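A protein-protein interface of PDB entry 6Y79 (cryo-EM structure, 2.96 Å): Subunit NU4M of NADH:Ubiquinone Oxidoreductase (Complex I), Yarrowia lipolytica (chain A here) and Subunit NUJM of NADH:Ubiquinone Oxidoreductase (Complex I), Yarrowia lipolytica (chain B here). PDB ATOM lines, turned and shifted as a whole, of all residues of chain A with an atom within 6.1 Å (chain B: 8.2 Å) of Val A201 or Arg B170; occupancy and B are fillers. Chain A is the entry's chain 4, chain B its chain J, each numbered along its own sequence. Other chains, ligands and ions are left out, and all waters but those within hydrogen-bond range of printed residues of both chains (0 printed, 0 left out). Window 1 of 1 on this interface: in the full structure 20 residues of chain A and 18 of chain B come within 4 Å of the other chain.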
ATOM      1  N   LEU A 189     -11.305  36.309  12.924  1.00  0.00           N
ATOM      2  CA  LEU A 189     -10.690  35.691  11.763  1.00  0.00           C
ATOM      3  C   LEU A 189     -10.009  36.707  10.869  1.00  0.00           C
ATOM      4  O   LEU A 189      -9.081  36.348  10.138  1.00  0.00           O
ATOM      5  CB  LEU A 189     -11.747  34.935  10.962  1.00  0.00           C
ATOM      6  CG  LEU A 189     -12.450  33.767  11.635  1.00  0.00           C
ATOM      7  CD1 LEU A 189     -13.434  33.150  10.671  1.00  0.00           C
ATOM      8  CD2 LEU A 189     -11.432  32.762  12.054  1.00  0.00           C
ATOM      9  N   HIS A 197     -13.722  29.146   5.159  1.00  0.00           N
ATOM     10  CA  HIS A 197     -14.130  29.272   6.548  1.00  0.00           C
ATOM     11  C   HIS A 197     -14.318  27.945   7.266  1.00  0.00           C
ATOM     12  O   HIS A 197     -14.487  27.949   8.485  1.00  0.00           O
ATOM     13  CB  HIS A 197     -15.390  30.133   6.631  1.00  0.00           C
ATOM     14  CG  HIS A 197     -16.618  29.509   6.048  1.00  0.00           C
ATOM     15  ND1 HIS A 197     -16.711  29.130   4.728  1.00  0.00           N
ATOM     16  CD2 HIS A 197     -17.824  29.248   6.596  1.00  0.00           C
ATOM     17  CE1 HIS A 197     -17.913  28.637   4.497  1.00  0.00           C
ATOM     18  NE2 HIS A 197     -18.614  28.720   5.610  1.00  0.00           N
ATOM     19  N   ASN A 198     -14.246  26.813   6.572  1.00  0.00           N
ATOM     20  CA  ASN A 198     -14.190  25.551   7.293  1.00  0.00           C
ATOM     21  C   ASN A 198     -12.782  25.211   7.759  1.00  0.00           C
ATOM     22  O   ASN A 198     -12.627  24.336   8.610  1.00  0.00           O
ATOM     23  CB  ASN A 198     -14.759  24.416   6.439  1.00  0.00           C
ATOM     24  CG  ASN A 198     -14.139  24.335   5.057  1.00  0.00           C
ATOM     25  OD1 ASN A 198     -13.213  25.066   4.723  1.00  0.00           O
ATOM     26  ND2 ASN A 198     -14.659  23.432   4.244  1.00  0.00           N
ATOM     27  N   LEU A 199     -11.759  25.887   7.229  1.00  0.00           N
ATOM     28  CA  LEU A 199     -10.386  25.606   7.636  1.00  0.00           C
ATOM     29  C   LEU A 199     -10.075  26.174   9.009  1.00  0.00           C
ATOM     30  O   LEU A 199      -9.253  25.614   9.737  1.00  0.00           O
ATOM     31  CB  LEU A 199      -9.409  26.171   6.616  1.00  0.00           C
ATOM     32  CG  LEU A 199      -9.473  25.526   5.241  1.00  0.00           C
ATOM     33  CD1 LEU A 199      -8.688  26.336   4.238  1.00  0.00           C
ATOM     34  CD2 LEU A 199      -8.932  24.128   5.341  1.00  0.00           C
ATOM     35  N   PHE A 200     -10.715  27.274   9.377  1.00  0.00           N
ATOM     36  CA  PHE A 200     -10.480  27.913  10.660  1.00  0.00           C
ATOM     37  C   PHE A 200     -11.235  27.188  11.764  1.00  0.00           C
ATOM     38  O   PHE A 200     -12.410  26.856  11.609  1.00  0.00           O
ATOM     39  CB  PHE A 200     -10.928  29.370  10.596  1.00  0.00           C
ATOM     40  CG  PHE A 200     -10.164  30.201   9.602  1.00  0.00           C
ATOM     41  CD1 PHE A 200      -8.953  30.767   9.942  1.00  0.00           C
ATOM     42  CD2 PHE A 200     -10.653  30.415   8.333  1.00  0.00           C
ATOM     43  CE1 PHE A 200      -8.249  31.531   9.046  1.00  0.00           C
ATOM     44  CE2 PHE A 200      -9.945  31.176   7.426  1.00  0.00           C
ATOM     45  CZ  PHE A 200      -8.742  31.735   7.788  1.00  0.00           C
ATOM     46  N   VAL A 201     -10.560  26.936  12.881  1.00  0.00           N
ATOM     47  CA  VAL A 201     -11.170  26.308  14.048  1.00  0.00           C
ATOM     48  C   VAL A 201     -11.120  27.289  15.206  1.00  0.00           C
ATOM     49  O   VAL A 201     -10.040  27.739  15.597  1.00  0.00           O
ATOM     50  CB  VAL A 201     -10.468  24.997  14.435  1.00  0.00           C
ATOM     51  CG1 VAL A 201     -11.258  24.284  15.482  1.00  0.00           C
ATOM     52  CG2 VAL A 201     -10.278  24.117  13.246  1.00  0.00           C
ATOM     53  N   LEU A 202     -12.273  27.598  15.770  1.00  0.00           N
ATOM     54  CA  LEU A 202     -12.340  28.455  16.939  1.00  0.00           C
ATOM     55  C   LEU A 202     -12.362  27.607  18.201  1.00  0.00           C
ATOM     56  O   LEU A 202     -12.497  26.384  18.157  1.00  0.00           O
ATOM     57  CB  LEU A 202     -13.570  29.359  16.867  1.00  0.00           C
ATOM     58  CG  LEU A 202     -13.581  30.257  15.636  1.00  0.00           C
ATOM     59  CD1 LEU A 202     -14.920  30.932  15.438  1.00  0.00           C
ATOM     60  CD2 LEU A 202     -12.506  31.273  15.782  1.00  0.00           C
ATOM     61  N   SER A 203     -12.208  28.274  19.339  1.00  0.00           N
ATOM     62  CA  SER A 203     -12.329  27.594  20.615  1.00  0.00           C
ATOM     63  C   SER A 203     -13.774  27.165  20.823  1.00  0.00           C
ATOM     64  O   SER A 203     -14.688  27.691  20.191  1.00  0.00           O
ATOM     65  CB  SER A 203     -11.874  28.508  21.750  1.00  0.00           C
ATOM     66  OG  SER A 203     -11.979  27.862  23.002  1.00  0.00           O
ATOM     67  N   LEU A 204     -13.979  26.186  21.706  1.00  0.00           N
ATOM     68  CA  LEU A 204     -15.328  25.674  21.899  1.00  0.00           C
ATOM     69  C   LEU A 204     -16.230  26.718  22.545  1.00  0.00           C
ATOM     70  O   LEU A 204     -17.339  26.961  22.054  1.00  0.00           O
ATOM     71  CB  LEU A 204     -15.317  24.395  22.734  1.00  0.00           C
ATOM     72  CG  LEU A 204     -16.724  23.812  22.890  1.00  0.00           C
ATOM     73  CD1 LEU A 204     -17.259  23.335  21.556  1.00  0.00           C
ATOM     74  CD2 LEU A 204     -16.778  22.708  23.916  1.00  0.00           C
ATOM     75  N   GLN A 207     -16.955  29.463  20.021  1.00  0.00           N
ATOM     76  CA  GLN A 207     -17.950  28.968  19.079  1.00  0.00           C
ATOM     77  C   GLN A 207     -19.350  28.992  19.674  1.00  0.00           C
ATOM     78  O   GLN A 207     -20.307  29.369  18.997  1.00  0.00           O
ATOM     79  CB  GLN A 207     -17.604  27.551  18.637  1.00  0.00           C
ATOM     80  CG  GLN A 207     -16.691  27.459  17.453  1.00  0.00           C
ATOM     81  CD  GLN A 207     -16.397  26.030  17.109  1.00  0.00           C
ATOM     82  OE1 GLN A 207     -16.996  25.127  17.674  1.00  0.00           O
ATOM     83  NE2 GLN A 207     -15.464  25.810  16.205  1.00  0.00           N
ATOM     84  N   GLU A 268     -18.293  21.942  16.065  1.00  0.00           N
ATOM     85  CA  GLU A 268     -18.148  21.536  17.447  1.00  0.00           C
ATOM     86  C   GLU A 268     -19.119  22.270  18.361  1.00  0.00           C
ATOM     87  O   GLU A 268     -19.401  21.789  19.458  1.00  0.00           O
ATOM     88  CB  GLU A 268     -16.698  21.758  17.880  1.00  0.00           C
ATOM     89  CG  GLU A 268     -15.689  20.840  17.191  1.00  0.00           C
ATOM     90  CD  GLU A 268     -15.175  21.367  15.862  1.00  0.00           C
ATOM     91  OE1 GLU A 268     -15.513  22.505  15.493  1.00  0.00           O
ATOM     92  OE2 GLU A 268     -14.437  20.633  15.177  1.00  0.00           O
ATOM     93  N   TYR A 484     -20.391  16.024   9.877  1.00  0.00           N
ATOM     94  CA  TYR A 484     -19.299  16.018  10.851  1.00  0.00           C
ATOM     95  C   TYR A 484     -19.419  14.735  11.680  1.00  0.00           C
ATOM     96  O   TYR A 484     -19.933  14.745  12.797  1.00  0.00           O
ATOM     97  CB  TYR A 484     -19.397  17.288  11.704  1.00  0.00           C
ATOM     98  CG  TYR A 484     -18.274  17.518  12.673  1.00  0.00           C
ATOM     99  CD1 TYR A 484     -17.068  18.053  12.254  1.00  0.00           C
ATOM    100  CD2 TYR A 484     -18.427  17.218  14.018  1.00  0.00           C
ATOM    101  CE1 TYR A 484     -16.047  18.265  13.138  1.00  0.00           C
ATOM    102  CE2 TYR A 484     -17.407  17.422  14.910  1.00  0.00           C
ATOM    103  CZ  TYR A 484     -16.221  17.947  14.463  1.00  0.00           C
ATOM    104  OH  TYR A 484     -15.193  18.158  15.344  1.00  0.00           O
ATOM    105  N   GLY B 153      -5.129  35.586  16.537  1.00  0.00           N
ATOM    106  CA  GLY B 153      -4.591  35.059  15.303  1.00  0.00           C
ATOM    107  C   GLY B 153      -4.345  33.566  15.390  1.00  0.00           C
ATOM    108  O   GLY B 153      -4.868  32.866  16.256  1.00  0.00           O
ATOM    109  N   PHE B 154      -3.526  33.078  14.468  1.00  0.00           N
ATOM    110  CA  PHE B 154      -3.084  31.700  14.535  1.00  0.00           C
ATOM    111  C   PHE B 154      -2.133  31.494  15.704  1.00  0.00           C
ATOM    112  O   PHE B 154      -1.396  32.396  16.108  1.00  0.00           O
ATOM    113  CB  PHE B 154      -2.369  31.292  13.251  1.00  0.00           C
ATOM    114  CG  PHE B 154      -3.261  31.195  12.061  1.00  0.00           C
ATOM    115  CD1 PHE B 154      -4.203  30.189  11.966  1.00  0.00           C
ATOM    116  CD2 PHE B 154      -3.144  32.099  11.024  1.00  0.00           C
ATOM    117  CE1 PHE B 154      -5.021  30.097  10.866  1.00  0.00           C
ATOM    118  CE2 PHE B 154      -3.959  32.010   9.917  1.00  0.00           C
ATOM    119  CZ  PHE B 154      -4.898  31.009   9.839  1.00  0.00           C
ATOM    120  N   VAL B 155      -2.149  30.278  16.248  1.00  0.00           N
ATOM    121  CA  VAL B 155      -0.989  29.809  16.991  1.00  0.00           C
ATOM    122  C   VAL B 155       0.173  29.677  16.006  1.00  0.00           C
ATOM    123  O   VAL B 155      -0.025  29.369  14.822  1.00  0.00           O
ATOM    124  CB  VAL B 155      -1.310  28.490  17.725  1.00  0.00           C
ATOM    125  CG1 VAL B 155      -2.555  28.650  18.548  1.00  0.00           C
ATOM    126  CG2 VAL B 155      -1.522  27.342  16.763  1.00  0.00           C
ATOM    127  N   ASP B 158       2.409  24.591  17.771  1.00  0.00           N
ATOM    128  CA  ASP B 158       1.324  23.854  18.404  1.00  0.00           C
ATOM    129  C   ASP B 158       1.372  24.001  19.917  1.00  0.00           C
ATOM    130  O   ASP B 158       2.402  23.752  20.553  1.00  0.00           O
ATOM    131  CB  ASP B 158       1.387  22.384  18.001  1.00  0.00           C
ATOM    132  CG  ASP B 158       1.027  22.168  16.542  1.00  0.00           C
ATOM    133  OD1 ASP B 158       0.241  22.970  16.001  1.00  0.00           O
ATOM    134  OD2 ASP B 158       1.530  21.198  15.940  1.00  0.00           O
ATOM    135  N   GLN B 161      -4.619  25.876  22.481  1.00  0.00           N
ATOM    136  CA  GLN B 161      -5.299  26.970  21.797  1.00  0.00           C
ATOM    137  C   GLN B 161      -6.122  27.757  22.804  1.00  0.00           C
ATOM    138  O   GLN B 161      -7.025  27.212  23.445  1.00  0.00           O
ATOM    139  CB  GLN B 161      -6.184  26.435  20.676  1.00  0.00           C
ATOM    140  CG  GLN B 161      -7.193  27.443  20.168  1.00  0.00           C
ATOM    141  CD  GLN B 161      -8.095  26.888  19.104  1.00  0.00           C
ATOM    142  OE1 GLN B 161      -8.054  25.701  18.796  1.00  0.00           O
ATOM    143  NE2 GLN B 161      -8.910  27.748  18.519  1.00  0.00           N
ATOM    144  N   THR B 162      -5.796  29.028  22.968  1.00  0.00           N
ATOM    145  CA  THR B 162      -6.535  29.834  23.912  1.00  0.00           C
ATOM    146  C   THR B 162      -7.825  30.332  23.284  1.00  0.00           C
ATOM    147  O   THR B 162      -8.073  30.163  22.092  1.00  0.00           O
ATOM    148  CB  THR B 162      -5.697  31.015  24.381  1.00  0.00           C
ATOM    149  OG1 THR B 162      -5.672  32.028  23.379  1.00  0.00           O
ATOM    150  CG2 THR B 162      -4.282  30.568  24.687  1.00  0.00           C
ATOM    151  N   TRP B 164      -9.898  33.323  21.778  1.00  0.00           N
ATOM    152  CA  TRP B 164      -9.583  34.303  20.730  1.00  0.00           C
ATOM    153  C   TRP B 164      -8.573  33.799  19.706  1.00  0.00           C
ATOM    154  O   TRP B 164      -8.226  34.549  18.790  1.00  0.00           O
ATOM    155  CB  TRP B 164      -9.092  35.664  21.256  1.00  0.00           C
ATOM    156  CG  TRP B 164     -10.067  36.440  22.066  1.00  0.00           C
ATOM    157  CD1 TRP B 164      -9.947  36.781  23.370  1.00  0.00           C
ATOM    158  CD2 TRP B 164     -11.306  36.994  21.619  1.00  0.00           C
ATOM    159  NE1 TRP B 164     -11.037  37.502  23.773  1.00  0.00           N
ATOM    160  CE2 TRP B 164     -11.886  37.650  22.710  1.00  0.00           C
ATOM    161  CE3 TRP B 164     -11.978  37.002  20.401  1.00  0.00           C
ATOM    162  CZ2 TRP B 164     -13.107  38.299  22.621  1.00  0.00           C
ATOM    163  CZ3 TRP B 164     -13.184  37.649  20.314  1.00  0.00           C
ATOM    164  CH2 TRP B 164     -13.737  38.287  21.413  1.00  0.00           C
ATOM    165  N   GLU B 165      -8.113  32.556  19.802  1.00  0.00           N
ATOM    166  CA  GLU B 165      -7.133  32.019  18.868  1.00  0.00           C
ATOM    167  C   GLU B 165      -7.752  31.025  17.898  1.00  0.00           C
ATOM    168  O   GLU B 165      -8.749  30.364  18.195  1.00  0.00           O
ATOM    169  CB  GLU B 165      -5.985  31.333  19.592  1.00  0.00           C
ATOM    170  CG  GLU B 165      -4.925  32.274  20.099  1.00  0.00           C
ATOM    171  CD  GLU B 165      -3.848  31.550  20.865  1.00  0.00           C
ATOM    172  OE1 GLU B 165      -3.951  30.319  20.992  1.00  0.00           O
ATOM    173  OE2 GLU B 165      -2.903  32.206  21.342  1.00  0.00           O
ATOM    174  N   VAL B 166      -7.133  30.926  16.730  1.00  0.00           N
ATOM    175  CA  VAL B 166      -7.584  30.065  15.651  1.00  0.00           C
ATOM    176  C   VAL B 166      -6.470  29.078  15.332  1.00  0.00           C
ATOM    177  O   VAL B 166      -5.290  29.429  15.358  1.00  0.00           O
ATOM    178  CB  VAL B 166      -7.955  30.911  14.413  1.00  0.00           C
ATOM    179  CG1 VAL B 166      -8.517  30.062  13.344  1.00  0.00           C
ATOM    180  CG2 VAL B 166      -8.945  31.988  14.770  1.00  0.00           C
ATOM    181  N   VAL B 167      -6.838  27.828  15.052  1.00  0.00           N
ATOM    182  CA  VAL B 167      -5.920  26.845  14.509  1.00  0.00           C
ATOM    183  C   VAL B 167      -6.484  26.334  13.189  1.00  0.00           C
ATOM    184  O   VAL B 167      -7.549  26.749  12.747  1.00  0.00           O
ATOM    185  CB  VAL B 167      -5.665  25.677  15.479  1.00  0.00           C
ATOM    186  CG1 VAL B 167      -5.091  26.177  16.776  1.00  0.00           C
ATOM    187  CG2 VAL B 167      -6.935  24.931  15.733  1.00  0.00           C
ATOM    188  N   HIS B 168      -5.736  25.438  12.551  1.00  0.00           N
ATOM    189  CA  HIS B 168      -6.203  24.729  11.369  1.00  0.00           C
ATOM    190  C   HIS B 168      -6.827  23.391  11.739  1.00  0.00           C
ATOM    191  O   HIS B 168      -7.876  23.022  11.210  1.00  0.00           O
ATOM    192  CB  HIS B 168      -5.052  24.501  10.392  1.00  0.00           C
ATOM    193  CG  HIS B 168      -4.606  25.730   9.668  1.00  0.00           C
ATOM    194  ND1 HIS B 168      -3.516  26.470  10.067  1.00  0.00           N
ATOM    195  CD2 HIS B 168      -5.089  26.337   8.560  1.00  0.00           C
ATOM    196  CE1 HIS B 168      -3.350  27.485   9.239  1.00  0.00           C
ATOM    197  NE2 HIS B 168      -4.293  27.429   8.317  1.00  0.00           N
ATOM    198  N   ARG B 169      -6.178  22.651  12.632  1.00  0.00           N
ATOM    199  CA  ARG B 169      -6.678  21.390  13.152  1.00  0.00           C
ATOM    200  C   ARG B 169      -6.615  21.416  14.666  1.00  0.00           C
ATOM    201  O   ARG B 169      -5.635  21.885  15.248  1.00  0.00           O
ATOM    202  CB  ARG B 169      -5.870  20.203  12.650  1.00  0.00           C
ATOM    203  CG  ARG B 169      -6.010  19.919  11.184  1.00  0.00           C
ATOM    204  CD  ARG B 169      -5.025  18.859  10.760  1.00  0.00           C
ATOM    205  NE  ARG B 169      -5.458  17.532  11.169  1.00  0.00           N
ATOM    206  CZ  ARG B 169      -6.122  16.702  10.379  1.00  0.00           C
ATOM    207  NH1 ARG B 169      -6.417  17.073   9.149  1.00  0.00           N
ATOM    208  NH2 ARG B 169      -6.494  15.510  10.815  1.00  0.00           N
ATOM    209  N   ARG B 170      -7.567  20.936  15.242  1.00  0.00           N
ATOM    210  CA  ARG B 170      -7.888  20.705  16.632  1.00  0.00           C
ATOM    211  C   ARG B 170      -7.434  19.311  17.034  1.00  0.00           C
ATOM    212  O   ARG B 170      -7.362  18.426  16.188  1.00  0.00           O
ATOM    213  CB  ARG B 170      -9.398  20.829  16.831  1.00  0.00           C
ATOM    214  CG  ARG B 170      -9.835  21.201  18.201  1.00  0.00           C
ATOM    215  CD  ARG B 170     -11.229  21.769  18.171  1.00  0.00           C
ATOM    216  NE  ARG B 170     -11.885  21.581  19.449  1.00  0.00           N
ATOM    217  CZ  ARG B 170     -12.606  20.511  19.725  1.00  0.00           C
ATOM    218  NH1 ARG B 170     -12.746  19.576  18.804  1.00  0.00           N
ATOM    219  NH2 ARG B 170     -13.179  20.374  20.902  1.00  0.00           N
ATOM    220  N   PRO B 171      -7.086  19.043  18.288  1.00  0.00           N
ATOM    221  CA  PRO B 171      -6.835  17.652  18.686  1.00  0.00           C
ATOM    222  C   PRO B 171      -8.127  16.856  18.817  1.00  0.00           C
ATOM    223  O   PRO B 171      -9.134  17.350  19.328  1.00  0.00           O
ATOM    224  CB  PRO B 171      -6.127  17.792  20.040  1.00  0.00           C
ATOM    225  CG  PRO B 171      -6.412  19.164  20.497  1.00  0.00           C
ATOM    226  CD  PRO B 171      -6.547  19.994  19.271  1.00  0.00           C
ATOM    227  N   LEU B 172      -8.086  15.601  18.347  1.00  0.00           N
ATOM    228  CA  LEU B 172      -9.270  14.741  18.380  1.00  0.00           C
ATOM    229  C   LEU B 172      -9.618  14.309  19.796  1.00  0.00           C
ATOM    230  O   LEU B 172     -10.782  14.005  20.083  1.00  0.00           O
ATOM    231  CB  LEU B 172      -9.055  13.512  17.496  1.00  0.00           C
ATOM    232  CG  LEU B 172     -10.240  12.676  17.005  1.00  0.00           C
ATOM    233  CD1 LEU B 172      -9.971  12.183  15.603  1.00  0.00           C
ATOM    234  CD2 LEU B 172     -10.489  11.495  17.908  1.00  0.00           C
ATOM    235  N   SER B 173      -8.626  14.255  20.684  1.00  0.00           N
ATOM    236  CA  SER B 173      -8.887  13.935  22.083  1.00  0.00           C
ATOM    237  C   SER B 173      -9.696  15.033  22.752  1.00  0.00           C
ATOM    238  O   SER B 173     -10.558  14.760  23.596  1.00  0.00           O
ATOM    239  CB  SER B 173      -7.568  13.724  22.818  1.00  0.00           C
ATOM    240  OG  SER B 173      -6.864  12.624  22.280  1.00  0.00           O
ATOM    241  N   LEU B 174      -9.440  16.283  22.366  1.00  0.00           N
ATOM    242  CA  LEU B 174     -10.246  17.407  22.819  1.00  0.00           C
ATOM    243  C   LEU B 174     -11.668  17.326  22.279  1.00  0.00           C
ATOM    244  O   LEU B 174     -12.617  17.707  22.974  1.00  0.00           O
ATOM    245  CB  LEU B 174      -9.568  18.698  22.379  1.00  0.00           C
ATOM    246  CG  LEU B 174     -10.023  20.075  22.849  1.00  0.00           C
ATOM    247  CD1 LEU B 174      -9.779  20.241  24.316  1.00  0.00           C
ATOM    248  CD2 LEU B 174      -9.288  21.142  22.069  1.00  0.00           C
ATOM    249  N   THR B 175     -11.833  16.814  21.058  1.00  0.00           N
ATOM    250  CA  THR B 175     -13.160  16.626  20.484  1.00  0.00           C
ATOM    251  C   THR B 175     -13.935  15.552  21.231  1.00  0.00           C
ATOM    252  O   THR B 175     -15.136  15.696  21.471  1.00  0.00           O
ATOM    253  CB  THR B 175     -13.033  16.263  19.006  1.00  0.00           C
ATOM    254  OG1 THR B 175     -12.042  17.097  18.405  1.00  0.00           O
ATOM    255  CG2 THR B 175     -14.325  16.501  18.292  1.00  0.00           C
ATOM    256  N   VAL B 176     -13.260  14.467  21.607  1.00  0.00           N
ATOM    257  CA  VAL B 176     -13.936  13.390  22.320  1.00  0.00           C
ATOM    258  C   VAL B 176     -14.266  13.810  23.750  1.00  0.00           C
ATOM    259  O   VAL B 176     -15.343  13.494  24.272  1.00  0.00           O
ATOM    260  CB  VAL B 176     -13.076  12.115  22.253  1.00  0.00           C
ATOM    261  CG1 VAL B 176     -13.587  11.033  23.190  1.00  0.00           C
ATOM    262  CG2 VAL B 176     -13.055  11.598  20.830  1.00  0.00           C
ATOM    263  N   GLU B 177     -13.386  14.585  24.385  1.00  0.00           N
ATOM    264  CA  GLU B 177     -13.647  15.002  25.759  1.00  0.00           C
ATOM    265  C   GLU B 177     -14.697  16.102  25.841  1.00  0.00           C
ATOM    266  O   GLU B 177     -15.483  16.137  26.794  1.00  0.00           O
ATOM    267  CB  GLU B 177     -12.363  15.474  26.429  1.00  0.00           C
ATOM    268  CG  GLU B 177     -11.387  14.369  26.724  1.00  0.00           C
ATOM    269  CD  GLU B 177     -10.140  14.872  27.412  1.00  0.00           C
ATOM    270  OE1 GLU B 177     -10.000  16.105  27.556  1.00  0.00           O
ATOM    271  OE2 GLU B 177      -9.301  14.036  27.808  1.00  0.00           O
ATOM    272  N   GLN B 178     -14.728  17.012  24.869  1.00  0.00           N
ATOM    273  CA  GLN B 178     -15.645  18.141  24.932  1.00  0.00           C
ATOM    274  C   GLN B 178     -17.037  17.793  24.433  1.00  0.00           C
ATOM    275  O   GLN B 178     -18.030  18.174  25.058  1.00  0.00           O
ATOM    276  CB  GLN B 178     -15.092  19.311  24.120  1.00  0.00           C
ATOM    277  CG  GLN B 178     -13.986  20.072  24.811  1.00  0.00           C
ATOM    278  CD  GLN B 178     -13.522  21.247  23.998  1.00  0.00           C
ATOM    279  OE1 GLN B 178     -13.905  21.393  22.846  1.00  0.00           O
ATOM    280  NE2 GLN B 178     -12.701  22.098  24.591  1.00  0.00           N
ATOM    281  N   LEU B 179     -17.131  17.083  23.314  1.00  0.00           N
ATOM    282  CA  LEU B 179     -18.417  16.760  22.713  1.00  0.00           C
ATOM    283  C   LEU B 179     -18.986  15.463  23.277  1.00  0.00           C
ATOM    284  O   LEU B 179     -20.081  15.456  23.847  1.00  0.00           O
ATOM    285  CB  LEU B 179     -18.267  16.673  21.194  1.00  0.00           C
ATOM    286  CG  LEU B 179     -18.031  18.009  20.509  1.00  0.00           C
ATOM    287  CD1 LEU B 179     -17.701  17.861  19.048  1.00  0.00           C
ATOM    288  CD2 LEU B 179     -19.273  18.780  20.649  1.00  0.00           C
ATOM    289  N   GLY B 180     -18.258  14.374  23.133  1.00  0.00           N
ATOM    290  CA  GLY B 180     -18.732  13.083  23.588  1.00  0.00           C
ATOM    291  C   GLY B 180     -18.239  11.991  22.662  1.00  0.00           C
ATOM    292  O   GLY B 180     -17.495  12.227  21.720  1.00  0.00           O
ATOM    293  N   ILE B 185     -19.555  10.624  16.542  1.00  0.00           N
ATOM    294  CA  ILE B 185     -18.270  11.076  17.042  1.00  0.00           C
ATOM    295  C   ILE B 185     -17.588   9.925  17.769  1.00  0.00           C
ATOM    296  O   ILE B 185     -18.207   9.227  18.581  1.00  0.00           O
ATOM    297  CB  ILE B 185     -18.452  12.322  17.926  1.00  0.00           C
ATOM    298  CG1 ILE B 185     -17.133  12.803  18.485  1.00  0.00           C
ATOM    299  CG2 ILE B 185     -19.509  12.132  19.009  1.00  0.00           C
ATOM    300  CD1 ILE B 185     -17.178  14.232  18.707  1.00  0.00           C
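Among the printed residues, pairs that only touch across the chains: Glu A268 with Leu B179 (3.2 Å), Leu A204 with Gln B178 (3.3 Å), Val A201 with His B168 (3.3 Å), Val A201 with Val B166 (3.4 Å), Leu A202 with Gln B161 (3.5 Å), Phe A200 with Phe B154 (3.5 Å), Tyr A484 with Thr B175 (3.5 Å), Phe A200 with Val B166 (3.5 Å), Glu A268 with Arg B170 (3.6 Å), Leu A199 with Val B167 (3.6 Å), Val A201 with Arg B170 (3.7 Å), Leu A189 with Val B166 (3.8 Å), Leu A202 with Val B166 (3.8 Å), Phe A200 with Val B167 (3.8 Å) and Val A201 with Glu B165 (3.9 Å).
Hydrophobic or aromatic side chains of chain B that line the printed part of chain A: Phe B154, Val B166, Val B167 and Leu B179.
Of the 12 printed residues of chain A, 9 touch a printed residue of chain B.
Among the printed residues, 19 pairs touch across the chains.
The backbone NH (N) of Thr B162 is in hydrogen-bond range of the side-chain carboxylate (OE1) of Glu B165 (3.0 Å).
The side-chain carboxylate (OE2) of Glu A268 is in hydrogen-bond range of the side-chain hydroxyl (OH) of Tyr A484 (2.6 Å).
The side-chain hydroxyl of Thr B175 sits at hydrogen-bond distance from the guanidinium group of Arg B170 (2.6 Å).
The backbone carbonyl oxygen of Glu B165 sits at hydrogen-bond distance from the side-chain amide nitrogen of Gln B161, 2.6 Å away.
The backbone carbonyl oxygen (O) of Gly B153 is in hydrogen-bond range of the backbone NH (N) of Val B166, 3.0 Å away.
The guanidinium group (NH2) of Arg B170 lies within hydrogen-bond range of the backbone carbonyl oxygen (O) of Leu B174.
Of chain A, only Val A201 and Glu A268 come within 4 Å of Arg B170.
Of the printed residues of chain A, Gln B178 touches Leu A204 (3.3 Å).
Printed residues of chain A within 4 Å of Glu B165: Val A201 (3.9 Å).
Printed residues of chain A within 4 Å of Leu B179: Glu A268 (3.2 Å).
Of the printed residues of chain B, Glu A268 touches Arg B170 and Leu B179.
Printed residues of chain A within 4 Å of Phe B154: Phe A200.
Val B176 touches none of the printed residues of chain A.
The nearest residue of chain A that does not touch Arg B170 is Tyr A484 (4.5 Å).
The backbone carbonyl oxygen (O) of His B168 lies close to the backbone carbonyl oxygen (O) of Leu A199, 3.3 Å away.
N of Ser A203 sits close to NE2 of Gln B161 (3.4 Å).
The backbone carbonyl oxygen (O) of Val B167 lies within hydrogen-bond range of the backbone NH (N) of Val A201, at 3.0 Å.
O of Val A201 sits at hydrogen-bond distance from NE2 of Gln B161 (3.1 Å).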
